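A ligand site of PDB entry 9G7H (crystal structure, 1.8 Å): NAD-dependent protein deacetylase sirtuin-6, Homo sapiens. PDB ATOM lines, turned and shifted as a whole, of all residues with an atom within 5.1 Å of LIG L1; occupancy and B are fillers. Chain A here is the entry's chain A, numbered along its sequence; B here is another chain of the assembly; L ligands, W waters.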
ATOM      1  N   GLY A  46     -22.264 -12.937  20.676  1.00  0.00           N
ATOM      2  CA  GLY A  46     -21.669 -14.002  19.916  1.00  0.00           C
ATOM      3  C   GLY A  46     -20.176 -13.760  19.707  1.00  0.00           C
ATOM      4  O   GLY A  46     -19.545 -12.999  20.466  1.00  0.00           O
ATOM      5  N   ALA A  47     -19.706 -14.424  18.641  1.00  0.00           N
ATOM      6  CA  ALA A  47     -18.298 -14.703  18.483  1.00  0.00           C
ATOM      7  C   ALA A  47     -17.511 -13.392  18.367  1.00  0.00           C
ATOM      8  O   ALA A  47     -16.351 -13.354  18.810  1.00  0.00           O
ATOM      9  CB  ALA A  47     -18.099 -15.669  17.288  1.00  0.00           C
ATOM     10  N   GLY A  48     -18.122 -12.287  17.848  1.00  0.00           N
ATOM     11  CA  GLY A  48     -17.417 -10.996  17.631  1.00  0.00           C
ATOM     12  C   GLY A  48     -16.881 -10.335  18.923  1.00  0.00           C
ATOM     13  O   GLY A  48     -15.972  -9.497  18.817  1.00  0.00           O
ATOM     14  N   THR A  51     -13.108 -11.812  19.395  1.00  0.00           N
ATOM     15  CA  THR A  51     -12.103 -11.638  18.365  1.00  0.00           C
ATOM     16  C   THR A  51     -10.949 -10.803  18.932  1.00  0.00           C
ATOM     17  O   THR A  51      -9.801 -11.003  18.542  1.00  0.00           O
ATOM     18  CB  THR A  51     -12.667 -11.007  17.093  1.00  0.00           C
ATOM     19  OG1 THR A  51     -13.252  -9.765  17.384  1.00  0.00           O
ATOM     20  CG2 THR A  51     -13.722 -11.849  16.391  1.00  0.00           C
ATOM     21  N   ASP A  57     -13.826 -15.413  14.755  1.00  0.00           N
ATOM     22  CA  ASP A  57     -15.281 -15.613  14.720  1.00  0.00           C
ATOM     23  C   ASP A  57     -15.606 -16.615  13.589  1.00  0.00           C
ATOM     24  O   ASP A  57     -14.709 -17.299  13.144  1.00  0.00           O
ATOM     25  CB  ASP A  57     -15.976 -14.263  14.578  1.00  0.00           C
ATOM     26  CG  ASP A  57     -15.730 -13.450  13.313  1.00  0.00           C
ATOM     27  OD1 ASP A  57     -15.262 -14.065  12.326  1.00  0.00           O
ATOM     28  OD2 ASP A  57     -16.116 -12.259  13.304  1.00  0.00           O
ATOM     29  N   PHE A  58     -16.895 -16.788  13.197  1.00  0.00           N
ATOM     30  CA  PHE A  58     -17.264 -17.744  12.165  1.00  0.00           C
ATOM     31  C   PHE A  58     -17.479 -17.122  10.777  1.00  0.00           C
ATOM     32  O   PHE A  58     -17.133 -17.774   9.747  1.00  0.00           O
ATOM     33  CB  PHE A  58     -18.550 -18.446  12.654  1.00  0.00           C
ATOM     34  CG  PHE A  58     -18.333 -19.267  13.901  1.00  0.00           C
ATOM     35  CD1 PHE A  58     -17.820 -20.560  13.807  1.00  0.00           C
ATOM     36  CD2 PHE A  58     -18.570 -18.688  15.150  1.00  0.00           C
ATOM     37  CE1 PHE A  58     -17.620 -21.272  14.993  1.00  0.00           C
ATOM     38  CE2 PHE A  58     -18.435 -19.437  16.299  1.00  0.00           C
ATOM     39  CZ  PHE A  58     -17.964 -20.718  16.188  1.00  0.00           C
ATOM     40  N   ARG A  59     -18.091 -15.913  10.735  1.00  0.00           N
ATOM     41  CA  ARG A  59     -18.667 -15.339   9.504  1.00  0.00           C
ATOM     42  C   ARG A  59     -18.058 -13.978   9.149  1.00  0.00           C
ATOM     43  O   ARG A  59     -18.404 -13.360   8.126  1.00  0.00           O
ATOM     44  CB  ARG A  59     -20.203 -15.333   9.535  1.00  0.00           C
ATOM     45  CG  ARG A  59     -20.783 -16.743   9.483  1.00  0.00           C
ATOM     46  CD  ARG A  59     -22.263 -16.797   9.463  1.00  0.00           C
ATOM     47  NE  ARG A  59     -22.757 -18.112   9.831  1.00  0.00           N
ATOM     48  CZ  ARG A  59     -22.766 -18.691  11.034  1.00  0.00           C
ATOM     49  NH1 ARG A  59     -22.454 -17.993  12.127  1.00  0.00           N
ATOM     50  NH2 ARG A  59     -23.116 -19.957  11.142  1.00  0.00           N
ATOM     51  N   GLY A  60     -17.160 -13.457  10.019  1.00  0.00           N
ATOM     52  CA  GLY A  60     -16.413 -12.252   9.714  1.00  0.00           C
ATOM     53  C   GLY A  60     -15.459 -12.423   8.527  1.00  0.00           C
ATOM     54  O   GLY A  60     -15.354 -13.509   7.977  1.00  0.00           O
ATOM     55  N   TRP A  65     -15.772 -20.141   9.081  1.00  0.00           N
ATOM     56  CA  TRP A  65     -16.510 -20.547   7.891  1.00  0.00           C
ATOM     57  C   TRP A  65     -16.142 -19.732   6.637  1.00  0.00           C
ATOM     58  O   TRP A  65     -15.988 -20.283   5.547  1.00  0.00           O
ATOM     59  CB  TRP A  65     -18.039 -20.527   8.128  1.00  0.00           C
ATOM     60  CG  TRP A  65     -18.596 -21.277   9.300  1.00  0.00           C
ATOM     61  CD1 TRP A  65     -19.752 -20.903   9.943  1.00  0.00           C
ATOM     62  CD2 TRP A  65     -18.137 -22.465   9.976  1.00  0.00           C
ATOM     63  NE1 TRP A  65     -20.047 -21.774  10.947  1.00  0.00           N
ATOM     64  CE2 TRP A  65     -19.072 -22.736  11.004  1.00  0.00           C
ATOM     65  CE3 TRP A  65     -17.040 -23.322   9.816  1.00  0.00           C
ATOM     66  CZ2 TRP A  65     -18.923 -23.813  11.879  1.00  0.00           C
ATOM     67  CZ3 TRP A  65     -16.876 -24.382  10.691  1.00  0.00           C
ATOM     68  CH2 TRP A  65     -17.808 -24.615  11.718  1.00  0.00           C
ATOM     69  N   GLN A 107     -24.077 -17.345  22.416  1.00  0.00           N
ATOM     70  CA  GLN A 107     -23.945 -18.428  21.474  1.00  0.00           C
ATOM     71  C   GLN A 107     -22.533 -18.997  21.555  1.00  0.00           C
ATOM     72  O   GLN A 107     -22.234 -20.020  20.918  1.00  0.00           O
ATOM     73  CB  GLN A 107     -24.276 -17.947  20.045  1.00  0.00           C
ATOM     74  CG  GLN A 107     -25.741 -17.590  19.791  1.00  0.00           C
ATOM     75  CD  GLN A 107     -25.968 -16.905  18.466  1.00  0.00           C
ATOM     76  OE1 GLN A 107     -25.867 -17.524  17.403  1.00  0.00           O
ATOM     77  NE2 GLN A 107     -26.355 -15.630  18.511  1.00  0.00           N
ATOM     78  N   ASN A 108     -21.646 -18.316  22.332  1.00  0.00           N
ATOM     79  CA  ASN A 108     -20.234 -18.641  22.385  1.00  0.00           C
ATOM     80  C   ASN A 108     -19.969 -19.899  23.200  1.00  0.00           C
ATOM     81  O   ASN A 108     -20.591 -20.109  24.280  1.00  0.00           O
ATOM     82  CB  ASN A 108     -19.414 -17.473  22.938  1.00  0.00           C
ATOM     83  CG  ASN A 108     -19.504 -16.274  22.028  1.00  0.00           C
ATOM     84  OD1 ASN A 108     -20.125 -16.317  20.961  1.00  0.00           O
ATOM     85  ND2 ASN A 108     -19.029 -15.147  22.534  1.00  0.00           N
ATOM     86  N   HIS A 127     -25.088 -22.854  22.947  1.00  0.00           N
ATOM     87  CA  HIS A 127     -24.384 -23.801  22.095  1.00  0.00           C
ATOM     88  C   HIS A 127     -23.338 -24.605  22.871  1.00  0.00           C
ATOM     89  O   HIS A 127     -22.615 -25.487  22.321  1.00  0.00           O
ATOM     90  CB  HIS A 127     -23.812 -23.070  20.871  1.00  0.00           C
ATOM     91  CG  HIS A 127     -24.799 -22.263  20.037  1.00  0.00           C
ATOM     92  ND1 HIS A 127     -24.422 -21.400  19.029  1.00  0.00           N
ATOM     93  CD2 HIS A 127     -26.148 -22.349  19.951  1.00  0.00           C
ATOM     94  CE1 HIS A 127     -25.492 -20.821  18.507  1.00  0.00           C
ATOM     95  NE2 HIS A 127     -26.562 -21.466  18.976  1.00  0.00           N
ATOM     96  N   TRP A 182     -24.426 -29.775  14.753  1.00  0.00           N
ATOM     97  CA  TRP A 182     -25.439 -29.170  13.902  1.00  0.00           C
ATOM     98  C   TRP A 182     -26.851 -29.698  14.161  1.00  0.00           C
ATOM     99  O   TRP A 182     -27.794 -28.917  14.185  1.00  0.00           O
ATOM    100  CB  TRP A 182     -25.055 -29.376  12.428  1.00  0.00           C
ATOM    101  CG  TRP A 182     -23.923 -28.480  12.012  1.00  0.00           C
ATOM    102  CD1 TRP A 182     -22.606 -28.806  11.929  1.00  0.00           C
ATOM    103  CD2 TRP A 182     -24.026 -27.078  11.696  1.00  0.00           C
ATOM    104  NE1 TRP A 182     -21.875 -27.699  11.558  1.00  0.00           N
ATOM    105  CE2 TRP A 182     -22.714 -26.623  11.422  1.00  0.00           C
ATOM    106  CE3 TRP A 182     -25.082 -26.160  11.627  1.00  0.00           C
ATOM    107  CZ2 TRP A 182     -22.444 -25.302  11.082  1.00  0.00           C
ATOM    108  CZ3 TRP A 182     -24.807 -24.847  11.284  1.00  0.00           C
ATOM    109  CH2 TRP A 182     -23.510 -24.428  11.025  1.00  0.00           C
ATOM    110  N   GLY A 208     -21.669  -8.446  18.595  1.00  0.00           N
ATOM    111  CA  GLY A 208     -20.845  -9.421  17.864  1.00  0.00           C
ATOM    112  C   GLY A 208     -21.558 -10.714  17.483  1.00  0.00           C
ATOM    113  O   GLY A 208     -20.976 -11.758  17.664  1.00  0.00           O
ATOM    114  N   THR A 209     -22.809 -10.620  17.015  1.00  0.00           N
ATOM    115  CA  THR A 209     -23.510 -11.786  16.441  1.00  0.00           C
ATOM    116  C   THR A 209     -24.255 -11.377  15.177  1.00  0.00           C
ATOM    117  O   THR A 209     -24.953 -10.349  15.172  1.00  0.00           O
ATOM    118  CB  THR A 209     -24.497 -12.415  17.438  1.00  0.00           C
ATOM    119  OG1 THR A 209     -25.242 -13.354  16.681  1.00  0.00           O
ATOM    120  CG2 THR A 209     -25.399 -11.376  18.068  1.00  0.00           C
ATOM    121  N   SER A 210     -24.081 -12.169  14.101  1.00  0.00           N
ATOM    122  CA  SER A 210     -24.762 -11.961  12.829  1.00  0.00           C
ATOM    123  C   SER A 210     -26.252 -12.357  12.899  1.00  0.00           C
ATOM    124  O   SER A 210     -26.971 -12.081  11.944  1.00  0.00           O
ATOM    125  CB  SER A 210     -24.046 -12.722  11.725  1.00  0.00           C
ATOM    126  OG  SER A 210     -23.962 -14.100  11.988  1.00  0.00           O
ATOM    127  N   LEU A 211     -26.668 -13.005  13.997  1.00  0.00           N
ATOM    128  CA  LEU A 211     -28.101 -13.360  14.234  1.00  0.00           C
ATOM    129  C   LEU A 211     -28.690 -14.331  13.171  1.00  0.00           C
ATOM    130  O   LEU A 211     -29.904 -14.400  12.894  1.00  0.00           O
ATOM    131  CB  LEU A 211     -28.899 -12.074  14.348  1.00  0.00           C
ATOM    132  CG  LEU A 211     -28.532 -11.129  15.495  1.00  0.00           C
ATOM    133  CD1 LEU A 211     -29.229  -9.791  15.382  1.00  0.00           C
ATOM    134  CD2 LEU A 211     -28.808 -11.845  16.805  1.00  0.00           C
ATOM    135  N   GLN A 212     -27.862 -15.237  12.651  1.00  0.00           N
ATOM    136  CA  GLN A 212     -28.206 -16.086  11.524  1.00  0.00           C
ATOM    137  C   GLN A 212     -28.687 -17.484  11.941  1.00  0.00           C
ATOM    138  O   GLN A 212     -29.278 -18.163  11.108  1.00  0.00           O
ATOM    139  CB  GLN A 212     -27.038 -16.253  10.539  1.00  0.00           C
ATOM    140  CG  GLN A 212     -26.497 -14.982   9.921  1.00  0.00           C
ATOM    141  CD  GLN A 212     -25.639 -15.224   8.687  1.00  0.00           C
ATOM    142  OE1 GLN A 212     -25.978 -15.999   7.793  1.00  0.00           O
ATOM    143  NE2 GLN A 212     -24.514 -14.508   8.576  1.00  0.00           N
ATOM    144  N   ILE A 213     -28.439 -17.910  13.192  1.00  0.00           N
ATOM    145  CA  ILE A 213     -28.757 -19.227  13.707  1.00  0.00           C
ATOM    146  C   ILE A 213     -30.094 -19.144  14.446  1.00  0.00           C
ATOM    147  O   ILE A 213     -30.263 -18.284  15.293  1.00  0.00           O
ATOM    148  CB  ILE A 213     -27.634 -19.769  14.610  1.00  0.00           C
ATOM    149  CG1 ILE A 213     -26.293 -19.897  13.900  1.00  0.00           C
ATOM    150  CG2 ILE A 213     -28.053 -21.093  15.266  1.00  0.00           C
ATOM    151  CD1 ILE A 213     -26.250 -20.956  12.796  1.00  0.00           C
ATOM    152  N   VAL A 233     -25.235  -4.134  17.936  1.00  0.00           N
ATOM    153  CA  VAL A 233     -23.838  -3.667  17.760  1.00  0.00           C
ATOM    154  C   VAL A 233     -23.123  -4.740  16.946  1.00  0.00           C
ATOM    155  O   VAL A 233     -23.072  -5.907  17.404  1.00  0.00           O
ATOM    156  CB  VAL A 233     -23.132  -3.364  19.091  1.00  0.00           C
ATOM    157  CG1 VAL A 233     -21.721  -2.793  18.898  1.00  0.00           C
ATOM    158  CG2 VAL A 233     -23.942  -2.440  19.997  1.00  0.00           C
ATOM    159  N   ASN A 234     -22.534  -4.389  15.796  1.00  0.00           N
ATOM    160  CA  ASN A 234     -21.943  -5.372  14.878  1.00  0.00           C
ATOM    161  C   ASN A 234     -21.243  -4.685  13.705  1.00  0.00           C
ATOM    162  O   ASN A 234     -21.801  -3.718  13.155  1.00  0.00           O
ATOM    163  CB  ASN A 234     -22.960  -6.384  14.355  1.00  0.00           C
ATOM    164  CG  ASN A 234     -22.353  -7.734  14.070  1.00  0.00           C
ATOM    165  OD1 ASN A 234     -21.802  -8.390  14.976  1.00  0.00           O
ATOM    166  ND2 ASN A 234     -22.423  -8.211  12.835  1.00  0.00           N
ATOM    167  N   LEU A 235     -20.050  -5.152  13.338  1.00  0.00           N
ATOM    168  CA  LEU A 235     -19.280  -4.566  12.236  1.00  0.00           C
ATOM    169  C   LEU A 235     -19.902  -4.911  10.871  1.00  0.00           C
ATOM    170  O   LEU A 235     -19.829  -4.091   9.954  1.00  0.00           O
ATOM    171  CB  LEU A 235     -17.834  -5.041  12.324  1.00  0.00           C
ATOM    172  CG  LEU A 235     -16.950  -4.297  13.322  1.00  0.00           C
ATOM    173  CD1 LEU A 235     -15.653  -5.047  13.470  1.00  0.00           C
ATOM    174  CD2 LEU A 235     -16.704  -2.881  12.801  1.00  0.00           C
ATOM    175  N   GLN A 236     -20.556  -6.073  10.757  1.00  0.00           N
ATOM    176  CA  GLN A 236     -21.140  -6.537   9.500  1.00  0.00           C
ATOM    177  C   GLN A 236     -22.664  -6.447   9.595  1.00  0.00           C
ATOM    178  O   GLN A 236     -23.199  -6.280  10.701  1.00  0.00           O
ATOM    179  CB  GLN A 236     -20.852  -8.012   9.233  1.00  0.00           C
ATOM    180  CG  GLN A 236     -19.493  -8.328   8.638  1.00  0.00           C
ATOM    181  CD  GLN A 236     -19.273  -9.827   8.533  1.00  0.00           C
ATOM    182  OE1 GLN A 236     -19.933 -10.636   9.202  1.00  0.00           O
ATOM    183  NE2 GLN A 236     -18.336 -10.220   7.686  1.00  0.00           N
ATOM    184  N   PRO A 237     -23.402  -6.542   8.468  1.00  0.00           N
ATOM    185  CA  PRO A 237     -24.856  -6.646   8.545  1.00  0.00           C
ATOM    186  C   PRO A 237     -25.297  -7.869   9.331  1.00  0.00           C
ATOM    187  O   PRO A 237     -24.561  -8.836   9.429  1.00  0.00           O
ATOM    188  CB  PRO A 237     -25.274  -6.752   7.064  1.00  0.00           C
ATOM    189  CG  PRO A 237     -24.120  -6.100   6.318  1.00  0.00           C
ATOM    190  CD  PRO A 237     -22.898  -6.512   7.092  1.00  0.00           C
ATOM    191  N   GLY A 250     -19.325  -0.700  14.742  1.00  0.00           N
ATOM    192  CA  GLY A 250     -18.000  -0.407  15.255  1.00  0.00           C
ATOM    193  C   GLY A 250     -17.492  -1.555  16.122  1.00  0.00           C
ATOM    194  O   GLY A 250     -18.245  -2.493  16.362  1.00  0.00           O
ATOM    195  N   TYR A 251     -16.237  -1.457  16.578  1.00  0.00           N
ATOM    196  CA  TYR A 251     -15.658  -2.472  17.452  1.00  0.00           C
ATOM    197  C   TYR A 251     -16.342  -2.431  18.831  1.00  0.00           C
ATOM    198  O   TYR A 251     -16.482  -1.350  19.443  1.00  0.00           O
ATOM    199  CB  TYR A 251     -14.139  -2.288  17.573  1.00  0.00           C
ATOM    200  CG  TYR A 251     -13.369  -2.373  16.255  1.00  0.00           C
ATOM    201  CD1 TYR A 251     -12.901  -3.607  15.782  1.00  0.00           C
ATOM    202  CD2 TYR A 251     -13.187  -1.245  15.447  1.00  0.00           C
ATOM    203  CE1 TYR A 251     -12.252  -3.715  14.565  1.00  0.00           C
ATOM    204  CE2 TYR A 251     -12.532  -1.346  14.219  1.00  0.00           C
ATOM    205  CZ  TYR A 251     -12.084  -2.576  13.774  1.00  0.00           C
ATOM    206  OH  TYR A 251     -11.418  -2.712  12.588  1.00  0.00           O
ATOM    207  N   VAL A 252     -16.690  -3.643  19.339  1.00  0.00           N
ATOM    208  CA  VAL A 252     -17.568  -3.772  20.487  1.00  0.00           C
ATOM    209  C   VAL A 252     -16.855  -3.209  21.727  1.00  0.00           C
ATOM    210  O   VAL A 252     -17.466  -2.536  22.522  1.00  0.00           O
ATOM    211  CB  VAL A 252     -18.223  -5.162  20.717  1.00  0.00           C
ATOM    212  CG1 VAL A 252     -19.238  -5.478  19.635  1.00  0.00           C
ATOM    213  CG2 VAL A 252     -17.242  -6.322  20.846  1.00  0.00           C
ATOM    214  N   ASP B  77      -8.956  -6.429  15.049  1.00  0.00           N
ATOM    215  CA  ASP B  77     -10.109  -6.720  15.883  1.00  0.00           C
ATOM    216  C   ASP B  77     -10.336  -5.568  16.869  1.00  0.00           C
ATOM    217  O   ASP B  77     -11.164  -5.705  17.766  1.00  0.00           O
ATOM    218  CB  ASP B  77      -9.917  -8.076  16.541  1.00  0.00           C
ATOM    219  CG  ASP B  77      -9.682  -9.181  15.534  1.00  0.00           C
ATOM    220  OD1 ASP B  77     -10.624  -9.423  14.699  1.00  0.00           O
ATOM    221  OD2 ASP B  77      -8.584  -9.804  15.576  1.00  0.00           O
HETATM  222  N1  LIG L   1     -16.692  -5.604  17.047  1.00  0.00           N
HETATM  223  C1  LIG L   1     -17.911  -5.732  16.498  1.00  0.00           C
HETATM  224  N2  LIG L   1     -18.407  -6.718  15.759  1.00  0.00           N
HETATM  225  C2  LIG L   1     -17.477  -7.656  15.556  1.00  0.00           C
HETATM  226  C3  LIG L   1     -16.183  -7.677  16.033  1.00  0.00           C
HETATM  227  C4  LIG L   1     -15.784  -6.588  16.848  1.00  0.00           C
HETATM  228  N3  LIG L   1     -14.564  -6.470  17.361  1.00  0.00           N
HETATM  229  N4  LIG L   1     -15.543  -8.829  15.634  1.00  0.00           N
HETATM  230  C5  LIG L   1     -16.432  -9.470  14.901  1.00  0.00           C
HETATM  231  N5  LIG L   1     -17.621  -8.806  14.829  1.00  0.00           N
HETATM  232  P1  LIG L   1     -20.699 -14.868  13.485  1.00  0.00           P
HETATM  233  P2  LIG L   1     -22.187 -15.857  15.757  1.00  0.00           P
HETATM  234  C6  LIG L   1     -18.845  -9.247  14.186  1.00  0.00           C
HETATM  235  O1  LIG L   1     -21.784 -15.408  12.660  1.00  0.00           O
HETATM  236  O2  LIG L   1     -21.859 -15.982  17.219  1.00  0.00           O
HETATM  237  C7  LIG L   1     -21.757 -20.795  14.320  1.00  0.00           C
HETATM  238  O3  LIG L   1     -22.001 -21.918  13.531  1.00  0.00           O
HETATM  239  C8  LIG L   1     -18.663  -9.800  12.777  1.00  0.00           C
HETATM  240  O4  LIG L   1     -18.793  -8.785  11.816  1.00  0.00           O
HETATM  241  O5  LIG L   1     -19.284 -15.018  13.093  1.00  0.00           O
HETATM  242  O6  LIG L   1     -23.245 -14.937  15.325  1.00  0.00           O
HETATM  243  C9  LIG L   1     -21.513 -21.180  15.787  1.00  0.00           C
HETATM  244  O7  LIG L   1     -22.245 -22.304  16.260  1.00  0.00           O
HETATM  245  C10 LIG L   1     -19.796 -10.830  12.675  1.00  0.00           C
HETATM  246  O8  LIG L   1     -20.899 -10.351  11.953  1.00  0.00           O
HETATM  247  O9  LIG L   1     -20.841 -15.466  14.974  1.00  0.00           O
HETATM  248  C11 LIG L   1     -21.933 -19.932  16.518  1.00  0.00           C
HETATM  249  O10 LIG L   1     -22.215 -20.233  17.890  1.00  0.00           O
HETATM  250  C12 LIG L   1     -20.209 -11.117  14.128  1.00  0.00           C
HETATM  251  O11 LIG L   1     -19.365 -10.289  14.957  1.00  0.00           O
HETATM  252  C13 LIG L   1     -23.168 -19.526  15.714  1.00  0.00           C
HETATM  253  O12 LIG L   1     -22.891 -19.945  14.339  1.00  0.00           O
HETATM  254  C14 LIG L   1     -20.072 -12.540  14.537  1.00  0.00           C
HETATM  255  O13 LIG L   1     -21.014 -13.314  13.759  1.00  0.00           O
HETATM  256  C15 LIG L   1     -23.539 -18.070  15.698  1.00  0.00           C
HETATM  257  O14 LIG L   1     -22.426 -17.306  15.154  1.00  0.00           O
HETATM  258  C1  LG2 L   2      -8.088 -24.692  18.871  1.00  0.00           C
HETATM  259  C2  LG2 L   2      -9.754 -25.138  17.208  1.00  0.00           C
HETATM  260  C3  LG2 L   2      -7.964 -25.463  21.163  1.00  0.00           C
HETATM  261  C4  LG2 L   2      -7.424 -24.698  20.085  1.00  0.00           C
HETATM  262  C5  LG2 L   2     -11.234 -25.472  17.068  1.00  0.00           C
HETATM  263  C6  LG2 L   2      -6.305 -23.852  20.076  1.00  0.00           C
HETATM  264  N1  LG2 L   2     -22.408 -25.659  19.074  1.00  0.00           N
HETATM  265  N2  LG2 L   2     -24.641 -24.796  14.785  1.00  0.00           N
HETATM  266  C7  LG2 L   2     -14.255 -22.242  18.430  1.00  0.00           C
HETATM  267  C8  LG2 L   2     -16.518 -25.109  18.122  1.00  0.00           C
HETATM  268  C9  LG2 L   2     -18.049 -25.355  18.447  1.00  0.00           C
HETATM  269  C10 LG2 L   2     -18.954 -24.327  17.791  1.00  0.00           C
HETATM  270  C11 LG2 L   2     -20.398 -24.798  18.106  1.00  0.00           C
HETATM  271  C12 LG2 L   2     -22.546 -25.220  17.765  1.00  0.00           C
HETATM  272  C13 LG2 L   2     -23.663 -25.167  16.961  1.00  0.00           C
HETATM  273  C14 LG2 L   2     -23.498 -24.881  15.584  1.00  0.00           C
HETATM  274  C15 LG2 L   2     -24.976 -25.413  17.411  1.00  0.00           C
HETATM  275  C16 LG2 L   2     -26.121 -25.322  16.625  1.00  0.00           C
HETATM  276  C17 LG2 L   2     -25.960 -25.018  15.286  1.00  0.00           C
HETATM  277  N3  LG2 L   2     -21.399 -24.670  17.271  1.00  0.00           N
HETATM  278  O1  LG2 L   2     -20.960 -25.448  19.371  1.00  0.00           O
HETATM  279  O2  LG2 L   2     -15.956 -25.799  17.228  1.00  0.00           O
HETATM  280  N4  LG2 L   2     -15.831 -24.154  18.834  1.00  0.00           N
HETATM  281  C18 LG2 L   2     -14.359 -23.844  18.638  1.00  0.00           C
HETATM  282  O3  LG2 L   2     -14.721 -21.455  19.304  1.00  0.00           O
HETATM  283  N5  LG2 L   2     -13.716 -21.757  17.233  1.00  0.00           N
HETATM  284  C19 LG2 L   2     -13.559 -20.265  17.013  1.00  0.00           C
HETATM  285  C20 LG2 L   2     -14.938 -19.664  16.707  1.00  0.00           C
HETATM  286  C21 LG2 L   2     -15.548 -18.798  17.811  1.00  0.00           C
HETATM  287  C22 LG2 L   2     -13.642 -24.745  17.624  1.00  0.00           C
HETATM  288  N6  LG2 L   2     -12.137 -24.598  17.674  1.00  0.00           N
HETATM  289  O4  LG2 L   2     -11.535 -26.471  16.403  1.00  0.00           O
HETATM  290  N7  LG2 L   2      -9.261 -25.455  18.607  1.00  0.00           N
HETATM  291  C23 LG2 L   2      -9.796 -26.202  19.613  1.00  0.00           C
HETATM  292  O5  LG2 L   2     -10.837 -26.856  19.483  1.00  0.00           O
HETATM  293  N8  LG2 L   2      -9.166 -26.228  20.927  1.00  0.00           N
HETATM  294  O6  LG2 L   2      -7.468 -25.536  22.296  1.00  0.00           O
HETATM  295  O7  LG2 L   2      -5.122 -24.233  20.045  1.00  0.00           O
HETATM  296  N9  LG2 L   2      -6.686 -22.587  19.946  1.00  0.00           N
HETATM  297  O   HOH W   1     -13.040  -8.727  14.286  1.00  0.00           O
HETATM  298  O   HOH W   2     -16.487  -8.276  11.102  1.00  0.00           O
HETATM  299  O   HOH W   3     -13.777  -5.311  20.071  1.00  0.00           O
HETATM  300  O   HOH W   4     -25.040 -15.798  13.507  1.00  0.00           O
HETATM  301  O   HOH W   5     -20.806 -17.917  18.786  1.00  0.00           O
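The backbone NH (N) of Ser 210 sits at hydrogen-bond distance from an oxygen (O6) of LIG L1 (3.1 Å). The side-chain hydroxyl of Ser 210 lies within hydrogen-bond range of an oxygen (O1) of LIG L1, 2.6 Å away. An oxygen (O5) of LIG L1 is in hydrogen-bond range of the backbone NH of Arg 59, 2.8 Å away. The guanidinium group (NH1) of Arg 59 is in salt-bridge range of an oxygen (O1) of LIG L1 (2.7 Å). A ring nitrogen (ND1) of His 127 lies within hydrogen-bond range of an oxygen (O10) of LIG L1 (2.7 Å). An oxygen (O8) of LIG L1 sits at hydrogen-bond distance from the side-chain amide nitrogen of Asn 234 (2.8 Å). O6 of LIG L1 lies within hydrogen-bond range of OG1 of Thr 209 (2.9 Å). The backbone NH of Gln 236 sits close to an oxygen (O4) of LIG L1 (3.4 Å). An oxygen (O8) of LIG L1 sits at hydrogen-bond distance from the side-chain amide oxygen (OE1) of Gln 236. O of Gln 107 is in hydrogen-bond range of O10 of LIG L1 (3.0 Å). An oxygen (O5) of LIG L1 lies within hydrogen-bond range of the backbone NH of Phe 58. An oxygen (O2) of LIG L1 lies within hydrogen-bond range of the backbone NH of Ala 47 (3.0 Å). The backbone NH (N) of Val 252 lies within hydrogen-bond range of a nitrogen (N1) of LIG L1. N4 of LIG L1 lies within hydrogen-bond range of OG1 of Thr 51 (3.0 Å). An oxygen (O3) of LIG L1 is in hydrogen-bond range of the indole nitrogen of Trp 65, at 3.2 Å. N2 of LIG L1 is in hydrogen-bond range of N of Leu 235 (3.3 Å).
N3 of LG2 L2 sits at hydrogen-bond distance from O7 of LIG L1, 2.7 Å away.
The backbone carbonyl oxygen (O) of Arg 59 sits at hydrogen-bond distance from the side-chain amide nitrogen (NE2) of Gln 236. The backbone NH (N) of Thr 209 sits at hydrogen-bond distance from the side-chain amide oxygen (OD1) of Asn 234 (3.2 Å). The backbone NH (N) of Leu 211 lies within hydrogen-bond range of the side-chain hydroxyl (OG1) of Thr 209, 3.1 Å away. The backbone carbonyl oxygen (O) of Phe 58 is in hydrogen-bond range of the backbone NH (N) of Trp 65, at 2.8 Å. The backbone carbonyl oxygen (O) of Gly 48 sits at hydrogen-bond distance from the side-chain hydroxyl (OG1) of Thr 51 (3.1 Å). The backbone NH of Gly 48 sits at hydrogen-bond distance from the backbone carbonyl oxygen of Gly 208 (2.9 Å). The backbone NH of Gly 46 lies close to the backbone carbonyl oxygen of Gly 208 (3.5 Å). N of Gly 208 is in hydrogen-bond range of O of Val 233, 3.1 Å away.
A nitrogen (N4) of LIG L1 lies close to the backbone carbonyl oxygen of Gly 48, 3.3 Å away. The backbone carbonyl oxygen (O) of Gly 208 sits close to an oxygen (O11) of LIG L1 (3.5 Å). Merely in contact with LIG L1: Gly 46, Asp 57, Trp 182, Ile 213, Gly 250, Tyr 251 and Asp 77 of chain B. Hydrophobic or aromatic side chains that line LIG L1: Ala 47, Phe 58, Trp 65, His 127, Trp 182, Ile 213, Leu 235, Tyr 251 and Val 252.
Water W4 lies within hydrogen-bond range of OG of Ser 210 (2.5 Å), O6 of LIG L1 (2.7 Å), N of Gln 212 (3.0 Å) and N of Leu 211 (3.3 Å). Water W5 lies within hydrogen-bond range of an oxygen (O2) of LIG L1 (2.7 Å), the side-chain amide oxygen of Asn 108 (2.8 Å) and the backbone carbonyl oxygen of Gln 107 (3.3 Å). Water W1 lies within hydrogen-bond range of the side-chain carboxylate (OD1) of Asp 77 of chain B (2.5 Å), a nitrogen (N4) of LIG L1 (2.8 Å) and the side-chain hydroxyl (OG1) of Thr 51 (3.3 Å). Water W3 bridges a nitrogen (N3) of LIG L1 (3.1 Å) and the backbone NH of Val 252 (3.4 Å).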
